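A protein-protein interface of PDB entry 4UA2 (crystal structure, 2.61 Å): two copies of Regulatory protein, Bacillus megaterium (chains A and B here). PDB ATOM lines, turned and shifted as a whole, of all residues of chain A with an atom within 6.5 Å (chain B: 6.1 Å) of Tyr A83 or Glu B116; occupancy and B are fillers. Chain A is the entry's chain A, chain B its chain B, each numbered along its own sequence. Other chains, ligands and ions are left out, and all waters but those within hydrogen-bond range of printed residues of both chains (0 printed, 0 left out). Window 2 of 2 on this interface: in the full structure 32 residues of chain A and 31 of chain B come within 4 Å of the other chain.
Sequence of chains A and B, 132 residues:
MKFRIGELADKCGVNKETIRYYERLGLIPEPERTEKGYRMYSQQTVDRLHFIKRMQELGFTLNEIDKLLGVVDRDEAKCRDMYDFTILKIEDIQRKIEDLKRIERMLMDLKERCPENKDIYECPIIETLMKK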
ATOM      1  N   CYS A  79      14.446 -38.139 -16.842  1.00  0.00           N
ATOM      2  CA  CYS A  79      14.190 -36.759 -17.243  1.00  0.00           C
ATOM      3  C   CYS A  79      13.071 -36.139 -16.411  1.00  0.00           C
ATOM      4  O   CYS A  79      12.666 -35.002 -16.651  1.00  0.00           O
ATOM      5  CB  CYS A  79      13.842 -36.680 -18.730  1.00  0.00           C
ATOM      6  SG  CYS A  79      15.256 -36.873 -19.837  1.00  0.00           S
ATOM      7  N   ARG A  80      12.569 -36.895 -15.441  1.00  0.00           N
ATOM      8  CA  ARG A  80      11.495 -36.417 -14.575  1.00  0.00           C
ATOM      9  C   ARG A  80      11.964 -35.263 -13.693  1.00  0.00           C
ATOM     10  O   ARG A  80      13.084 -35.282 -13.180  1.00  0.00           O
ATOM     11  CB  ARG A  80      10.961 -37.559 -13.707  1.00  0.00           C
ATOM     12  N   ASP A  81      11.098 -34.265 -13.530  1.00  0.00           N
ATOM     13  CA  ASP A  81      11.378 -33.089 -12.702  1.00  0.00           C
ATOM     14  C   ASP A  81      12.658 -32.368 -13.125  1.00  0.00           C
ATOM     15  O   ASP A  81      13.539 -32.117 -12.305  1.00  0.00           O
ATOM     16  CB  ASP A  81      11.464 -33.485 -11.226  1.00  0.00           C
ATOM     17  N   MET A  82      12.749 -32.038 -14.408  1.00  0.00           N
ATOM     18  CA  MET A  82      13.927 -31.373 -14.957  1.00  0.00           C
ATOM     19  C   MET A  82      13.957 -29.875 -14.659  1.00  0.00           C
ATOM     20  O   MET A  82      15.025 -29.261 -14.624  1.00  0.00           O
ATOM     21  CB  MET A  82      14.000 -31.604 -16.467  1.00  0.00           C
ATOM     22  CG  MET A  82      14.918 -32.743 -16.871  1.00  0.00           C
ATOM     23  SD  MET A  82      16.787 -32.229 -16.722  1.00  0.00           S
ATOM     24  CE  MET A  82      16.702 -30.642 -17.834  1.00  0.00           C
ATOM     25  N   TYR A  83      12.780 -29.296 -14.446  1.00  0.00           N
ATOM     26  CA  TYR A  83      12.641 -27.862 -14.203  1.00  0.00           C
ATOM     27  C   TYR A  83      13.386 -27.418 -12.941  1.00  0.00           C
ATOM     28  O   TYR A  83      14.245 -26.529 -12.991  1.00  0.00           O
ATOM     29  CB  TYR A  83      11.155 -27.502 -14.103  1.00  0.00           C
ATOM     30  CG  TYR A  83      10.864 -26.023 -13.996  1.00  0.00           C
ATOM     31  CD1 TYR A  83      10.362 -25.480 -12.821  1.00  0.00           C
ATOM     32  CD2 TYR A  83      11.082 -25.171 -15.071  1.00  0.00           C
ATOM     33  CE1 TYR A  83      10.088 -24.130 -12.718  1.00  0.00           C
ATOM     34  CE2 TYR A  83      10.813 -23.819 -14.977  1.00  0.00           C
ATOM     35  CZ  TYR A  83      10.317 -23.304 -13.797  1.00  0.00           C
ATOM     36  OH  TYR A  83      10.046 -21.959 -13.695  1.00  0.00           O
ATOM     37  N   ASP A  84      13.054 -28.048 -11.818  1.00  0.00           N
ATOM     38  CA  ASP A  84      13.688 -27.742 -10.539  1.00  0.00           C
ATOM     39  C   ASP A  84      15.192 -27.985 -10.596  1.00  0.00           C
ATOM     40  O   ASP A  84      15.980 -27.207 -10.055  1.00  0.00           O
ATOM     41  CB  ASP A  84      13.060 -28.576  -9.421  1.00  0.00           C
ATOM     42  CG  ASP A  84      11.588 -28.270  -9.222  1.00  0.00           C
ATOM     43  OD1 ASP A  84      11.199 -27.094  -9.375  1.00  0.00           O
ATOM     44  OD2 ASP A  84      10.821 -29.206  -8.913  1.00  0.00           O
ATOM     45  N   PHE A  85      15.576 -29.073 -11.259  1.00  0.00           N
ATOM     46  CA  PHE A  85      16.980 -29.413 -11.456  1.00  0.00           C
ATOM     47  C   PHE A  85      17.720 -28.276 -12.153  1.00  0.00           C
ATOM     48  O   PHE A  85      18.761 -27.805 -11.674  1.00  0.00           O
ATOM     49  CB  PHE A  85      17.102 -30.706 -12.266  1.00  0.00           C
ATOM     50  CG  PHE A  85      18.518 -31.125 -12.537  1.00  0.00           C
ATOM     51  CD1 PHE A  85      19.100 -30.889 -13.772  1.00  0.00           C
ATOM     52  CD2 PHE A  85      19.267 -31.758 -11.559  1.00  0.00           C
ATOM     53  CE1 PHE A  85      20.402 -31.275 -14.025  1.00  0.00           C
ATOM     54  CE2 PHE A  85      20.569 -32.147 -11.807  1.00  0.00           C
ATOM     55  CZ  PHE A  85      21.138 -31.905 -13.040  1.00  0.00           C
ATOM     56  N   THR A  86      17.168 -27.832 -13.280  1.00  0.00           N
ATOM     57  CA  THR A  86      17.741 -26.719 -14.026  1.00  0.00           C
ATOM     58  C   THR A  86      17.844 -25.473 -13.163  1.00  0.00           C
ATOM     59  O   THR A  86      18.867 -24.802 -13.177  1.00  0.00           O
ATOM     60  CB  THR A  86      16.923 -26.382 -15.287  1.00  0.00           C
ATOM     61  OG1 THR A  86      15.532 -26.298 -14.955  1.00  0.00           O
ATOM     62  CG2 THR A  86      17.125 -27.442 -16.351  1.00  0.00           C
ATOM     63  N   ILE A  87      16.793 -25.167 -12.408  1.00  0.00           N
ATOM     64  CA  ILE A  87      16.813 -23.987 -11.542  1.00  0.00           C
ATOM     65  C   ILE A  87      17.959 -24.041 -10.525  1.00  0.00           C
ATOM     66  O   ILE A  87      18.756 -23.095 -10.416  1.00  0.00           O
ATOM     67  CB  ILE A  87      15.477 -23.820 -10.797  1.00  0.00           C
ATOM     68  CG1 ILE A  87      14.377 -23.410 -11.777  1.00  0.00           C
ATOM     69  CG2 ILE A  87      15.606 -22.784  -9.690  1.00  0.00           C
ATOM     70  CD1 ILE A  87      13.051 -23.112 -11.118  1.00  0.00           C
ATOM     71  N   LEU A  88      18.047 -25.153  -9.798  1.00  0.00           N
ATOM     72  CA  LEU A  88      19.109 -25.349  -8.813  1.00  0.00           C
ATOM     73  C   LEU A  88      20.496 -25.194  -9.434  1.00  0.00           C
ATOM     74  O   LEU A  88      21.324 -24.402  -8.958  1.00  0.00           O
ATOM     75  CB  LEU A  88      18.985 -26.729  -8.162  1.00  0.00           C
ATOM     76  CG  LEU A  88      17.737 -26.991  -7.316  1.00  0.00           C
ATOM     77  CD1 LEU A  88      17.704 -28.437  -6.844  1.00  0.00           C
ATOM     78  CD2 LEU A  88      17.680 -26.038  -6.134  1.00  0.00           C
ATOM     79  N   LYS B 111      15.574 -25.533 -19.385  1.00  0.00           N
ATOM     80  CA  LYS B 111      14.549 -24.931 -18.540  1.00  0.00           C
ATOM     81  C   LYS B 111      13.414 -24.344 -19.371  1.00  0.00           C
ATOM     82  O   LYS B 111      12.239 -24.567 -19.082  1.00  0.00           O
ATOM     83  CB  LYS B 111      15.162 -23.848 -17.651  1.00  0.00           C
ATOM     84  CG  LYS B 111      14.149 -23.002 -16.900  1.00  0.00           C
ATOM     85  CD  LYS B 111      14.844 -21.982 -16.013  1.00  0.00           C
ATOM     86  CE  LYS B 111      13.851 -21.011 -15.395  1.00  0.00           C
ATOM     87  NZ  LYS B 111      13.234 -20.121 -16.416  1.00  0.00           N
ATOM     88  N   CYS B 114      10.761 -26.608 -20.746  1.00  0.00           N
ATOM     89  CA  CYS B 114       9.783 -27.177 -19.819  1.00  0.00           C
ATOM     90  C   CYS B 114       8.478 -26.377 -19.813  1.00  0.00           C
ATOM     91  O   CYS B 114       8.493 -25.163 -20.011  1.00  0.00           O
ATOM     92  CB  CYS B 114      10.365 -27.242 -18.404  1.00  0.00           C
ATOM     93  SG  CYS B 114      11.842 -28.276 -18.247  1.00  0.00           S
ATOM     94  N   PRO B 115       7.343 -27.061 -19.593  1.00  0.00           N
ATOM     95  CA  PRO B 115       6.037 -26.393 -19.499  1.00  0.00           C
ATOM     96  C   PRO B 115       5.969 -25.409 -18.333  1.00  0.00           C
ATOM     97  O   PRO B 115       5.435 -24.304 -18.481  1.00  0.00           O
ATOM     98  CB  PRO B 115       5.060 -27.555 -19.284  1.00  0.00           C
ATOM     99  CG  PRO B 115       5.766 -28.752 -19.818  1.00  0.00           C
ATOM    100  CD  PRO B 115       7.215 -28.527 -19.520  1.00  0.00           C
ATOM    101  N   GLU B 116       6.525 -25.810 -17.193  1.00  0.00           N
ATOM    102  CA  GLU B 116       6.512 -24.999 -15.979  1.00  0.00           C
ATOM    103  C   GLU B 116       7.129 -23.619 -16.197  1.00  0.00           C
ATOM    104  O   GLU B 116       6.840 -22.677 -15.460  1.00  0.00           O
ATOM    105  CB  GLU B 116       7.249 -25.720 -14.846  1.00  0.00           C
ATOM    106  CG  GLU B 116       6.639 -27.055 -14.431  1.00  0.00           C
ATOM    107  CD  GLU B 116       7.032 -28.198 -15.351  1.00  0.00           C
ATOM    108  OE1 GLU B 116       7.781 -27.956 -16.321  1.00  0.00           O
ATOM    109  OE2 GLU B 116       6.591 -29.340 -15.103  1.00  0.00           O
ATOM    110  N   ASN B 117       7.979 -23.511 -17.213  1.00  0.00           N
ATOM    111  CA  ASN B 117       8.650 -22.258 -17.534  1.00  0.00           C
ATOM    112  C   ASN B 117       7.679 -21.174 -17.996  1.00  0.00           C
ATOM    113  O   ASN B 117       7.972 -19.982 -17.889  1.00  0.00           O
ATOM    114  CB  ASN B 117       9.716 -22.496 -18.604  1.00  0.00           C
ATOM    115  CG  ASN B 117      10.587 -21.281 -18.837  1.00  0.00           C
ATOM    116  OD1 ASN B 117      11.385 -20.902 -17.980  1.00  0.00           O
ATOM    117  ND2 ASN B 117      10.448 -20.668 -20.007  1.00  0.00           N
ATOM    118  N   LYS B 118       6.525 -21.587 -18.511  1.00  0.00           N
ATOM    119  CA  LYS B 118       5.512 -20.630 -18.948  1.00  0.00           C
ATOM    120  C   LYS B 118       4.559 -20.256 -17.817  1.00  0.00           C
ATOM    121  O   LYS B 118       3.769 -19.321 -17.942  1.00  0.00           O
ATOM    122  CB  LYS B 118       4.718 -21.193 -20.127  1.00  0.00           C
ATOM    123  CG  LYS B 118       5.567 -21.579 -21.321  1.00  0.00           C
ATOM    124  CD  LYS B 118       4.729 -22.226 -22.408  1.00  0.00           C
ATOM    125  CE  LYS B 118       5.610 -22.730 -23.534  1.00  0.00           C
ATOM    126  NZ  LYS B 118       6.610 -23.717 -23.041  1.00  0.00           N
ATOM    127  N   ASP B 119       4.642 -20.994 -16.714  1.00  0.00           N
ATOM    128  CA  ASP B 119       3.728 -20.819 -15.590  1.00  0.00           C
ATOM    129  C   ASP B 119       4.236 -19.793 -14.583  1.00  0.00           C
ATOM    130  O   ASP B 119       5.392 -19.840 -14.162  1.00  0.00           O
ATOM    131  CB  ASP B 119       3.487 -22.160 -14.897  1.00  0.00           C
ATOM    132  CG  ASP B 119       2.608 -23.088 -15.717  1.00  0.00           C
ATOM    133  OD1 ASP B 119       1.945 -22.599 -16.655  1.00  0.00           O
ATOM    134  OD2 ASP B 119       2.572 -24.301 -15.421  1.00  0.00           O
ATOM    135  N   ILE B 120       3.355 -18.876 -14.194  1.00  0.00           N
ATOM    136  CA  ILE B 120       3.724 -17.763 -13.327  1.00  0.00           C
ATOM    137  C   ILE B 120       4.065 -18.219 -11.906  1.00  0.00           C
ATOM    138  O   ILE B 120       5.015 -17.720 -11.304  1.00  0.00           O
ATOM    139  CB  ILE B 120       2.597 -16.697 -13.275  1.00  0.00           C
ATOM    140  CG1 ILE B 120       2.952 -15.590 -12.281  1.00  0.00           C
ATOM    141  CG2 ILE B 120       1.253 -17.330 -12.932  1.00  0.00           C
ATOM    142  CD1 ILE B 120       1.918 -14.496 -12.186  1.00  0.00           C
ATOM    143  N   GLU B 122       5.367 -20.887 -11.032  1.00  0.00           N
ATOM    144  CA  GLU B 122       6.576 -21.704 -11.046  1.00  0.00           C
ATOM    145  C   GLU B 122       7.844 -20.867 -11.184  1.00  0.00           C
ATOM    146  O   GLU B 122       8.943 -21.408 -11.287  1.00  0.00           O
ATOM    147  CB  GLU B 122       6.505 -22.736 -12.171  1.00  0.00           C
ATOM    148  CG  GLU B 122       5.563 -23.887 -11.878  1.00  0.00           C
ATOM    149  CD  GLU B 122       5.906 -24.591 -10.580  1.00  0.00           C
ATOM    150  OE1 GLU B 122       5.106 -24.499  -9.624  1.00  0.00           O
ATOM    151  OE2 GLU B 122       6.975 -25.235 -10.514  1.00  0.00           O
ATOM    152  N   CYS B 123       7.685 -19.548 -11.195  1.00  0.00           N
ATOM    153  CA  CYS B 123       8.827 -18.643 -11.276  1.00  0.00           C
ATOM    154  C   CYS B 123       9.675 -18.732 -10.008  1.00  0.00           C
ATOM    155  O   CYS B 123       9.149 -18.647  -8.901  1.00  0.00           O
ATOM    156  CB  CYS B 123       8.357 -17.206 -11.502  1.00  0.00           C
ATOM    157  SG  CYS B 123       9.684 -16.023 -11.826  1.00  0.00           S
ATOM    158  N   PRO B 124      10.993 -18.918 -10.170  1.00  0.00           N
ATOM    159  CA  PRO B 124      11.926 -19.039  -9.041  1.00  0.00           C
ATOM    160  C   PRO B 124      12.272 -17.697  -8.395  1.00  0.00           C
ATOM    161  O   PRO B 124      13.338 -17.144  -8.664  1.00  0.00           O
ATOM    162  CB  PRO B 124      13.165 -19.665  -9.684  1.00  0.00           C
ATOM    163  CG  PRO B 124      13.119 -19.202 -11.097  1.00  0.00           C
ATOM    164  CD  PRO B 124      11.664 -19.128 -11.466  1.00  0.00           C
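No position is printed for both chains.
Of the 10 printed residues of chain A, 3 touch a printed residue of chain B. Of the 11 printed residues of chain B, 6 touch a printed residue of chain A. Among the printed residues, 8 pairs touch across the chains. Among the printed residues, no Asp or Glu carboxylate lies within 4 Å of a Lys or Arg side-chain nitrogen of the other chain.
The backbone carbonyl oxygen of Glu B122 is in hydrogen-bond range of the side-chain hydroxyl of Tyr A83, 2.7 Å away.
The backbone carbonyl oxygen (O) of Met A82 is in hydrogen-bond range of the side-chain hydroxyl (OG1) of Thr A86. The side-chain amino group of Lys B111 is in hydrogen-bond range of the side-chain amide oxygen of Asn B117.
Among the printed residues, merely in contact across the chains: Tyr A83 with Lys B111 (3.9 Å), Tyr A83 with Cys B114 (3.99 Å), Tyr A83 with Glu B116 (3.7 Å), Tyr A83 with Asn B117 (3.6 Å), Tyr A83 with Pro B124 (3.9 Å), Thr A86 with Lys B111 (3.7 Å) and Ile A87 with Pro B124 (3.7 Å).
Of the printed residues of chain B, Tyr A83 touches Lys B111 (3.9 Å), Cys B114 (3.99 Å), Glu B116 (3.7 Å), Asn B117 (3.6 Å), Glu B122 (2.7 Å) and Pro B124 (3.9 Å). Of the printed residues of chain A, Glu B116 touches Tyr A83 (3.7 Å). Printed residues of chain A within 4 Å of Glu B122: Tyr A83 (2.7 Å). Printed residues of chain A within 4 Å of Lys B111: Tyr A83 and Thr A86. Of the printed residues of chain B, Ile A87 touches Pro B124 (3.7 Å). Of the printed residues of chain A, Pro B124 touches Tyr A83 (3.9 Å) and Ile A87 (3.7 Å). Of the printed residues of chain A, Asn B117 touches Tyr A83. Ile B120 touches none of the printed residues of chain A. Phe A85 touches none of the printed residues of chain B. The nearest printed residue of chain B that does not touch Tyr A83 is Cys B123 (4.2 Å). The nearest printed residue of chain A that does not touch Glu B116 is Asp A81 (6.5 Å).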
